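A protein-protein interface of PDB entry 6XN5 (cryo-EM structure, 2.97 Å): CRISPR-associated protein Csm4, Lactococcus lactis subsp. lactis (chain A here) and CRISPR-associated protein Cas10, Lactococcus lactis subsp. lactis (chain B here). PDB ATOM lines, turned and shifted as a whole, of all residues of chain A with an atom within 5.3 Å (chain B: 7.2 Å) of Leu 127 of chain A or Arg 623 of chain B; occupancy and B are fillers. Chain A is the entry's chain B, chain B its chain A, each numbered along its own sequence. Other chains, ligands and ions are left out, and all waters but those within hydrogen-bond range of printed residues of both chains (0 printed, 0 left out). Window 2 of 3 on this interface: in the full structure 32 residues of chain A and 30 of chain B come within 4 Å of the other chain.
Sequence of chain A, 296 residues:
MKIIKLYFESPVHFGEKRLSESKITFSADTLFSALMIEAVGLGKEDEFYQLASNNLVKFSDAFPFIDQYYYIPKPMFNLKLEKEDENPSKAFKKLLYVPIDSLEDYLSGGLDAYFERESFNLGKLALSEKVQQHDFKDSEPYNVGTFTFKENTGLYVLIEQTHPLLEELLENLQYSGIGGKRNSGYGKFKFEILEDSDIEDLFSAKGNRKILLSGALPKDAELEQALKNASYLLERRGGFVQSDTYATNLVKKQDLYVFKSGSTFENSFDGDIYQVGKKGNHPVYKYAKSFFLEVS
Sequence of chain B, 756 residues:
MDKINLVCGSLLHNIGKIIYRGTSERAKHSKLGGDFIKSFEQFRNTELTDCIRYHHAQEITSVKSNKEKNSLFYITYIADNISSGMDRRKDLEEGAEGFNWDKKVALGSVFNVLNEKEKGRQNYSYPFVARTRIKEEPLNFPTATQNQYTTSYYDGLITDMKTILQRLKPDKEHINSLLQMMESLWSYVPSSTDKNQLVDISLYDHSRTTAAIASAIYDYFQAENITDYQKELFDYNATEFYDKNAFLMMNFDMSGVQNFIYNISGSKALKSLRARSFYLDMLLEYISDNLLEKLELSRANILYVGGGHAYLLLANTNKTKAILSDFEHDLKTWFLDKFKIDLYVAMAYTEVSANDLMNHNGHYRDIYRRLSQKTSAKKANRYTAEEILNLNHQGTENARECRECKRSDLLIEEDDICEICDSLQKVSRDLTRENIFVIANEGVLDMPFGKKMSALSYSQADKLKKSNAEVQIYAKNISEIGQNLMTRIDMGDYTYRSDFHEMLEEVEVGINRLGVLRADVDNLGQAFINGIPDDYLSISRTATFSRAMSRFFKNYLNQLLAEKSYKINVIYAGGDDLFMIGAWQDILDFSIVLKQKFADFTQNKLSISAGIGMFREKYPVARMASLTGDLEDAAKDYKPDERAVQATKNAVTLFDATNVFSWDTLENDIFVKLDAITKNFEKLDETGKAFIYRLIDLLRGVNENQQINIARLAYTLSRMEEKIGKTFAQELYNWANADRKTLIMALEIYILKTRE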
ATOM      1  N   SER A  20      -4.979   6.086   5.480  1.00  0.00           N
ATOM      2  CA  SER A  20      -5.482   7.315   4.889  1.00  0.00           C
ATOM      3  C   SER A  20      -5.005   7.552   3.465  1.00  0.00           C
ATOM      4  O   SER A  20      -5.480   8.491   2.821  1.00  0.00           O
ATOM      5  CB  SER A  20      -5.078   8.509   5.754  1.00  0.00           C
ATOM      6  OG  SER A  20      -3.685   8.521   5.986  1.00  0.00           O
ATOM      7  N   GLU A  21      -4.088   6.740   2.960  1.00  0.00           N
ATOM      8  CA  GLU A  21      -3.464   6.945   1.664  1.00  0.00           C
ATOM      9  C   GLU A  21      -3.531   5.636   0.890  1.00  0.00           C
ATOM     10  O   GLU A  21      -3.444   4.555   1.467  1.00  0.00           O
ATOM     11  CB  GLU A  21      -2.014   7.411   1.863  1.00  0.00           C
ATOM     12  CG  GLU A  21      -1.192   7.733   0.614  1.00  0.00           C
ATOM     13  CD  GLU A  21      -1.716   8.930  -0.167  1.00  0.00           C
ATOM     14  OE1 GLU A  21      -2.370   9.807   0.435  1.00  0.00           O
ATOM     15  OE2 GLU A  21      -1.463   8.998  -1.386  1.00  0.00           O
ATOM     16  N   LEU A 125      -8.660   9.257  -6.661  1.00  0.00           N
ATOM     17  CA  LEU A 125      -8.591   8.930  -5.254  1.00  0.00           C
ATOM     18  C   LEU A 125      -9.715   9.612  -4.497  1.00  0.00           C
ATOM     19  O   LEU A 125     -10.345  10.554  -4.979  1.00  0.00           O
ATOM     20  CB  LEU A 125      -7.254   9.367  -4.670  1.00  0.00           C
ATOM     21  CG  LEU A 125      -6.008   8.693  -5.227  1.00  0.00           C
ATOM     22  CD1 LEU A 125      -4.782   9.396  -4.693  1.00  0.00           C
ATOM     23  CD2 LEU A 125      -5.993   7.230  -4.854  1.00  0.00           C
ATOM     24  N   ALA A 126      -9.954   9.133  -3.285  1.00  0.00           N
ATOM     25  CA  ALA A 126     -10.991   9.680  -2.436  1.00  0.00           C
ATOM     26  C   ALA A 126     -10.510   9.620  -0.998  1.00  0.00           C
ATOM     27  O   ALA A 126      -9.378   9.219  -0.719  1.00  0.00           O
ATOM     28  CB  ALA A 126     -12.300   8.915  -2.622  1.00  0.00           C
ATOM     29  N   LEU A 127     -11.370  10.035  -0.083  1.00  0.00           N
ATOM     30  CA  LEU A 127     -11.116   9.849   1.336  1.00  0.00           C
ATOM     31  C   LEU A 127     -12.460   9.669   2.014  1.00  0.00           C
ATOM     32  O   LEU A 127     -13.319  10.552   1.934  1.00  0.00           O
ATOM     33  CB  LEU A 127     -10.360  11.027   1.931  1.00  0.00           C
ATOM     34  CG  LEU A 127     -10.018  10.846   3.400  1.00  0.00           C
ATOM     35  CD1 LEU A 127      -8.730  10.094   3.525  1.00  0.00           C
ATOM     36  CD2 LEU A 127      -9.916  12.184   4.070  1.00  0.00           C
ATOM     37  N   SER A 128     -12.650   8.527   2.653  1.00  0.00           N
ATOM     38  CA  SER A 128     -13.862   8.265   3.400  1.00  0.00           C
ATOM     39  C   SER A 128     -13.687   8.787   4.814  1.00  0.00           C
ATOM     40  O   SER A 128     -12.631   8.604   5.418  1.00  0.00           O
ATOM     41  CB  SER A 128     -14.163   6.774   3.418  1.00  0.00           C
ATOM     42  OG  SER A 128     -15.413   6.511   4.019  1.00  0.00           O
ATOM     43  N   GLU A 129     -14.710   9.448   5.333  1.00  0.00           N
ATOM     44  CA  GLU A 129     -14.676   9.970   6.688  1.00  0.00           C
ATOM     45  C   GLU A 129     -15.553   9.111   7.582  1.00  0.00           C
ATOM     46  O   GLU A 129     -16.770   9.048   7.393  1.00  0.00           O
ATOM     47  CB  GLU A 129     -15.131  11.427   6.727  1.00  0.00           C
ATOM     48  CG  GLU A 129     -14.148  12.401   6.092  1.00  0.00           C
ATOM     49  CD  GLU A 129     -13.096  12.922   7.057  1.00  0.00           C
ATOM     50  OE1 GLU A 129     -12.666  14.079   6.878  1.00  0.00           O
ATOM     51  OE2 GLU A 129     -12.689  12.190   7.985  1.00  0.00           O
ATOM     52  N   ASN A 143     -10.016   8.053   9.085  1.00  0.00           N
ATOM     53  CA  ASN A 143     -10.231   8.329   7.677  1.00  0.00           C
ATOM     54  C   ASN A 143      -9.475   7.353   6.796  1.00  0.00           C
ATOM     55  O   ASN A 143      -8.293   7.083   7.010  1.00  0.00           O
ATOM     56  CB  ASN A 143      -9.871   9.781   7.386  1.00  0.00           C
ATOM     57  CG  ASN A 143      -8.594  10.209   8.062  1.00  0.00           C
ATOM     58  OD1 ASN A 143      -7.876   9.397   8.640  1.00  0.00           O
ATOM     59  ND2 ASN A 143      -8.349  11.506   8.070  1.00  0.00           N
ATOM     60  N   VAL A 144     -10.186   6.829   5.804  1.00  0.00           N
ATOM     61  CA  VAL A 144      -9.727   5.739   4.957  1.00  0.00           C
ATOM     62  C   VAL A 144      -9.583   6.268   3.542  1.00  0.00           C
ATOM     63  O   VAL A 144     -10.584   6.584   2.893  1.00  0.00           O
ATOM     64  CB  VAL A 144     -10.706   4.556   4.981  1.00  0.00           C
ATOM     65  CG1 VAL A 144     -10.237   3.465   4.067  1.00  0.00           C
ATOM     66  CG2 VAL A 144     -10.876   4.048   6.386  1.00  0.00           C
ATOM     67  N   GLY A 145      -8.350   6.353   3.056  1.00  0.00           N
ATOM     68  CA  GLY A 145      -8.133   6.786   1.693  1.00  0.00           C
ATOM     69  C   GLY A 145      -8.451   5.667   0.720  1.00  0.00           C
ATOM     70  O   GLY A 145      -7.966   4.545   0.849  1.00  0.00           O
ATOM     71  N   THR A 146      -9.289   5.980  -0.263  1.00  0.00           N
ATOM     72  CA  THR A 146      -9.736   4.985  -1.222  1.00  0.00           C
ATOM     73  C   THR A 146      -9.395   5.443  -2.630  1.00  0.00           C
ATOM     74  O   THR A 146      -8.733   6.459  -2.837  1.00  0.00           O
ATOM     75  CB  THR A 146     -11.240   4.698  -1.105  1.00  0.00           C
ATOM     76  OG1 THR A 146     -11.991   5.884  -1.368  1.00  0.00           O
ATOM     77  CG2 THR A 146     -11.591   4.187   0.260  1.00  0.00           C
ATOM     78  N   TYR B 262       6.654  14.927   3.725  1.00  0.00           N
ATOM     79  CA  TYR B 262       5.199  14.896   3.770  1.00  0.00           C
ATOM     80  C   TYR B 262       4.629  13.546   4.168  1.00  0.00           C
ATOM     81  O   TYR B 262       3.554  13.494   4.765  1.00  0.00           O
ATOM     82  CB  TYR B 262       4.637  15.319   2.418  1.00  0.00           C
ATOM     83  CG  TYR B 262       5.194  16.647   2.007  1.00  0.00           C
ATOM     84  CD1 TYR B 262       5.047  17.756   2.824  1.00  0.00           C
ATOM     85  CD2 TYR B 262       5.906  16.787   0.833  1.00  0.00           C
ATOM     86  CE1 TYR B 262       5.571  18.971   2.466  1.00  0.00           C
ATOM     87  CE2 TYR B 262       6.434  17.997   0.468  1.00  0.00           C
ATOM     88  CZ  TYR B 262       6.264  19.083   1.288  1.00  0.00           C
ATOM     89  OH  TYR B 262       6.796  20.292   0.922  1.00  0.00           O
ATOM     90  N   ASN B 263       5.317  12.452   3.873  1.00  0.00           N
ATOM     91  CA  ASN B 263       4.829  11.142   4.285  1.00  0.00           C
ATOM     92  C   ASN B 263       5.231  10.895   5.731  1.00  0.00           C
ATOM     93  O   ASN B 263       6.188  10.175   6.016  1.00  0.00           O
ATOM     94  CB  ASN B 263       5.356  10.055   3.363  1.00  0.00           C
ATOM     95  CG  ASN B 263       4.621  10.013   2.045  1.00  0.00           C
ATOM     96  OD1 ASN B 263       5.175  10.344   1.000  1.00  0.00           O
ATOM     97  ND2 ASN B 263       3.360   9.603   2.087  1.00  0.00           N
ATOM     98  N   PHE B 615      -8.394  22.822   3.350  1.00  0.00           N
ATOM     99  CA  PHE B 615      -8.561  21.578   4.086  1.00  0.00           C
ATOM    100  C   PHE B 615      -8.869  21.887   5.541  1.00  0.00           C
ATOM    101  O   PHE B 615      -8.626  22.991   6.024  1.00  0.00           O
ATOM    102  CB  PHE B 615      -7.303  20.704   4.049  1.00  0.00           C
ATOM    103  CG  PHE B 615      -6.742  20.490   2.687  1.00  0.00           C
ATOM    104  CD1 PHE B 615      -7.180  19.439   1.918  1.00  0.00           C
ATOM    105  CD2 PHE B 615      -5.778  21.339   2.171  1.00  0.00           C
ATOM    106  CE1 PHE B 615      -6.670  19.232   0.676  1.00  0.00           C
ATOM    107  CE2 PHE B 615      -5.259  21.127   0.918  1.00  0.00           C
ATOM    108  CZ  PHE B 615      -5.710  20.075   0.169  1.00  0.00           C
ATOM    109  N   ARG B 616      -9.371  20.885   6.253  1.00  0.00           N
ATOM    110  CA  ARG B 616      -9.456  20.979   7.699  1.00  0.00           C
ATOM    111  C   ARG B 616      -8.063  20.871   8.311  1.00  0.00           C
ATOM    112  O   ARG B 616      -7.101  20.468   7.656  1.00  0.00           O
ATOM    113  CB  ARG B 616     -10.350  19.881   8.257  1.00  0.00           C
ATOM    114  CG  ARG B 616     -11.741  19.841   7.681  1.00  0.00           C
ATOM    115  CD  ARG B 616     -12.516  18.651   8.222  1.00  0.00           C
ATOM    116  NE  ARG B 616     -12.030  17.383   7.684  1.00  0.00           N
ATOM    117  CZ  ARG B 616     -11.266  16.525   8.355  1.00  0.00           C
ATOM    118  NH1 ARG B 616     -10.894  16.797   9.596  1.00  0.00           N
ATOM    119  NH2 ARG B 616     -10.874  15.397   7.781  1.00  0.00           N
ATOM    120  N   LYS B 618      -7.312  18.805  10.774  1.00  0.00           N
ATOM    121  CA  LYS B 618      -7.078  17.392  11.036  1.00  0.00           C
ATOM    122  C   LYS B 618      -7.097  16.545   9.772  1.00  0.00           C
ATOM    123  O   LYS B 618      -7.297  15.328   9.846  1.00  0.00           O
ATOM    124  CB  LYS B 618      -8.098  16.875  12.047  1.00  0.00           C
ATOM    125  CG  LYS B 618      -7.925  17.493  13.417  1.00  0.00           C
ATOM    126  CD  LYS B 618      -6.546  17.187  13.967  1.00  0.00           C
ATOM    127  CE  LYS B 618      -6.363  17.761  15.358  1.00  0.00           C
ATOM    128  NZ  LYS B 618      -6.228  19.242  15.339  1.00  0.00           N
ATOM    129  N   TYR B 619      -6.891  17.159   8.613  1.00  0.00           N
ATOM    130  CA  TYR B 619      -6.778  16.410   7.380  1.00  0.00           C
ATOM    131  C   TYR B 619      -5.405  15.739   7.353  1.00  0.00           C
ATOM    132  O   TYR B 619      -4.460  16.250   7.956  1.00  0.00           O
ATOM    133  CB  TYR B 619      -6.953  17.356   6.197  1.00  0.00           C
ATOM    134  CG  TYR B 619      -7.273  16.692   4.889  1.00  0.00           C
ATOM    135  CD1 TYR B 619      -8.558  16.242   4.629  1.00  0.00           C
ATOM    136  CD2 TYR B 619      -6.306  16.505   3.921  1.00  0.00           C
ATOM    137  CE1 TYR B 619      -8.872  15.632   3.440  1.00  0.00           C
ATOM    138  CE2 TYR B 619      -6.612  15.892   2.726  1.00  0.00           C
ATOM    139  CZ  TYR B 619      -7.897  15.459   2.494  1.00  0.00           C
ATOM    140  OH  TYR B 619      -8.214  14.846   1.307  1.00  0.00           O
ATOM    141  N   PRO B 620      -5.279  14.566   6.726  1.00  0.00           N
ATOM    142  CA  PRO B 620      -3.967  13.903   6.672  1.00  0.00           C
ATOM    143  C   PRO B 620      -2.972  14.680   5.827  1.00  0.00           C
ATOM    144  O   PRO B 620      -3.253  15.034   4.684  1.00  0.00           O
ATOM    145  CB  PRO B 620      -4.284  12.544   6.045  1.00  0.00           C
ATOM    146  CG  PRO B 620      -5.696  12.337   6.281  1.00  0.00           C
ATOM    147  CD  PRO B 620      -6.349  13.671   6.263  1.00  0.00           C
ATOM    148  N   VAL B 621      -1.786  14.911   6.399  1.00  0.00           N
ATOM    149  CA  VAL B 621      -0.823  15.847   5.826  1.00  0.00           C
ATOM    150  C   VAL B 621      -0.219  15.303   4.531  1.00  0.00           C
ATOM    151  O   VAL B 621       0.071  16.066   3.601  1.00  0.00           O
ATOM    152  CB  VAL B 621       0.240  16.212   6.888  1.00  0.00           C
ATOM    153  CG1 VAL B 621       1.122  15.033   7.269  1.00  0.00           C
ATOM    154  CG2 VAL B 621       1.103  17.341   6.422  1.00  0.00           C
ATOM    155  N   ALA B 622      -0.070  13.981   4.424  1.00  0.00           N
ATOM    156  CA  ALA B 622       0.519  13.395   3.227  1.00  0.00           C
ATOM    157  C   ALA B 622      -0.446  13.471   2.059  1.00  0.00           C
ATOM    158  O   ALA B 622      -0.064  13.841   0.945  1.00  0.00           O
ATOM    159  CB  ALA B 622       0.919  11.949   3.497  1.00  0.00           C
ATOM    160  N   ARG B 623      -1.712  13.134   2.312  1.00  0.00           N
ATOM    161  CA  ARG B 623      -2.760  13.267   1.306  1.00  0.00           C
ATOM    162  C   ARG B 623      -2.984  14.727   0.935  1.00  0.00           C
ATOM    163  O   ARG B 623      -3.233  15.043  -0.234  1.00  0.00           O
ATOM    164  CB  ARG B 623      -4.041  12.610   1.834  1.00  0.00           C
ATOM    165  CG  ARG B 623      -5.288  12.933   1.063  1.00  0.00           C
ATOM    166  CD  ARG B 623      -6.364  11.892   1.240  1.00  0.00           C
ATOM    167  NE  ARG B 623      -7.455  12.135   0.302  1.00  0.00           N
ATOM    168  CZ  ARG B 623      -7.462  11.725  -0.961  1.00  0.00           C
ATOM    169  NH1 ARG B 623      -6.448  11.024  -1.445  1.00  0.00           N
ATOM    170  NH2 ARG B 623      -8.490  12.008  -1.742  1.00  0.00           N
ATOM    171  N   MET B 624      -2.843  15.620   1.915  1.00  0.00           N
ATOM    172  CA  MET B 624      -2.921  17.061   1.696  1.00  0.00           C
ATOM    173  C   MET B 624      -1.868  17.543   0.709  1.00  0.00           C
ATOM    174  O   MET B 624      -2.191  18.190  -0.295  1.00  0.00           O
ATOM    175  CB  MET B 624      -2.744  17.751   3.042  1.00  0.00           C
ATOM    176  CG  MET B 624      -3.346  19.080   3.191  1.00  0.00           C
ATOM    177  SD  MET B 624      -3.241  19.563   4.908  1.00  0.00           S
ATOM    178  CE  MET B 624      -1.472  19.580   5.050  1.00  0.00           C
ATOM    179  N   ALA B 625      -0.602  17.203   0.968  1.00  0.00           N
ATOM    180  CA  ALA B 625       0.482  17.620   0.084  1.00  0.00           C
ATOM    181  C   ALA B 625       0.384  16.939  -1.273  1.00  0.00           C
ATOM    182  O   ALA B 625       0.659  17.560  -2.304  1.00  0.00           O
ATOM    183  CB  ALA B 625       1.828  17.325   0.739  1.00  0.00           C
ATOM    184  N   SER B 626      -0.059  15.678  -1.295  1.00  0.00           N
ATOM    185  CA  SER B 626      -0.138  14.928  -2.542  1.00  0.00           C
ATOM    186  C   SER B 626      -1.219  15.479  -3.463  1.00  0.00           C
ATOM    187  O   SER B 626      -0.994  15.655  -4.665  1.00  0.00           O
ATOM    188  CB  SER B 626      -0.394  13.454  -2.246  1.00  0.00           C
ATOM    189  OG  SER B 626      -1.766  13.234  -1.976  1.00  0.00           O
ATOM    190  N   LEU B 627      -2.400  15.778  -2.926  1.00  0.00           N
ATOM    191  CA  LEU B 627      -3.403  16.277  -3.852  1.00  0.00           C
ATOM    192  C   LEU B 627      -3.251  17.770  -4.089  1.00  0.00           C
ATOM    193  O   LEU B 627      -3.710  18.260  -5.121  1.00  0.00           O
ATOM    194  CB  LEU B 627      -4.827  15.916  -3.406  1.00  0.00           C
ATOM    195  CG  LEU B 627      -5.635  16.288  -2.170  1.00  0.00           C
ATOM    196  CD1 LEU B 627      -6.265  17.627  -2.417  1.00  0.00           C
ATOM    197  CD2 LEU B 627      -6.689  15.251  -1.885  1.00  0.00           C
ATOM    198  N   THR B 628      -2.562  18.501  -3.208  1.00  0.00           N
ATOM    199  CA  THR B 628      -2.174  19.861  -3.563  1.00  0.00           C
ATOM    200  C   THR B 628      -1.179  19.836  -4.718  1.00  0.00           C
ATOM    201  O   THR B 628      -1.243  20.665  -5.629  1.00  0.00           O
ATOM    202  CB  THR B 628      -1.583  20.563  -2.345  1.00  0.00           C
ATOM    203  OG1 THR B 628      -2.537  20.527  -1.283  1.00  0.00           O
ATOM    204  CG2 THR B 628      -1.335  22.009  -2.655  1.00  0.00           C
ATOM    205  N   GLY B 629      -0.300  18.832  -4.733  1.00  0.00           N
ATOM    206  CA  GLY B 629       0.580  18.643  -5.871  1.00  0.00           C
ATOM    207  C   GLY B 629      -0.138  18.164  -7.120  1.00  0.00           C
ATOM    208  O   GLY B 629       0.328  18.403  -8.238  1.00  0.00           O
ATOM    209  N   ASP B 630      -1.266  17.464  -6.964  1.00  0.00           N
ATOM    210  CA  ASP B 630      -1.952  17.081  -8.198  1.00  0.00           C
ATOM    211  C   ASP B 630      -2.756  18.251  -8.767  1.00  0.00           C
ATOM    212  O   ASP B 630      -2.869  18.383  -9.988  1.00  0.00           O
ATOM    213  CB  ASP B 630      -2.728  15.746  -8.017  1.00  0.00           C
ATOM    214  CG  ASP B 630      -4.108  15.836  -7.309  1.00  0.00           C
ATOM    215  OD1 ASP B 630      -4.830  16.846  -7.264  1.00  0.00           O
ATOM    216  OD2 ASP B 630      -4.491  14.783  -6.758  1.00  0.00           O
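Of chain B, only Tyr 619 and Arg 623 come within 4 Å of Leu 127 of chain A.
Of chain A, only Ser 20 (3.9 Å), Glu 21 (3.6 Å), Leu 125 (3.7 Å), Ala 126 (3.1 Å) and Leu 127 (3.5 Å) come within 4 Å of Arg 623 of chain B.
Of the printed residues of chain B, Glu 21 of chain A touches Arg 623.
Of the printed residues of chain A, Arg 616 of chain B touches Glu 129 (2.4 Å).
Asn 263 of chain B touches none of the printed residues of chain A.
Gly 145 of chain A touches none of the printed residues of chain B.
The nearest residue of chain B that does not touch Leu 127 of chain A is Pro 620 of chain B (4.4 Å).
The nearest printed residue of chain B that does not touch Ser 20 of chain A is Ala 622 of chain B (6.3 Å).
Among the printed residues, merely in contact across the chains: Ser 20 of chain A with Pro 620 of chain B, Ser 20 of chain A with Arg 623 of chain B, Glu 21 of chain A with Arg 623 of chain B, Leu 125 of chain A with Arg 623 of chain B, Leu 127 of chain A with Tyr 619 of chain B, Leu 127 of chain A with Arg 623 of chain B and Asn 143 of chain A with Pro 620 of chain B.
Of the 17 printed residues of chain B, 4 touch a printed residue of chain A.
Hydrophobic or aromatic side chains of chain B within 4 Å of the printed part of chain A: Tyr 619 and Pro 620.
Among the printed residues, 9 pairs touch across the chains.
Among the printed residues, Asp or Glu carboxylates within 4 Å of a Lys or Arg side-chain nitrogen of the other chain: Glu 129 of chain A with Arg 616 of chain B.
NH2 of Arg 616 of chain B is in salt-bridge range of OE1 of Glu 129 of chain A (2.4 Å).
NH2 of Arg 623 of chain B is in hydrogen-bond range of O of Ala 126 of chain A, 3.1 Å away.
The side-chain hydroxyl of Tyr 619 of chain B sits at hydrogen-bond distance from the guanidinium group of Arg 623 of chain B, 3.0 Å away.
The side-chain hydroxyl of Ser 626 of chain B is in hydrogen-bond range of the backbone carbonyl oxygen of Arg 623 of chain B (2.9 Å).
The backbone NH (N) of Ala 126 of chain A lies within hydrogen-bond range of the backbone carbonyl oxygen (O) of Thr 146 of chain A.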
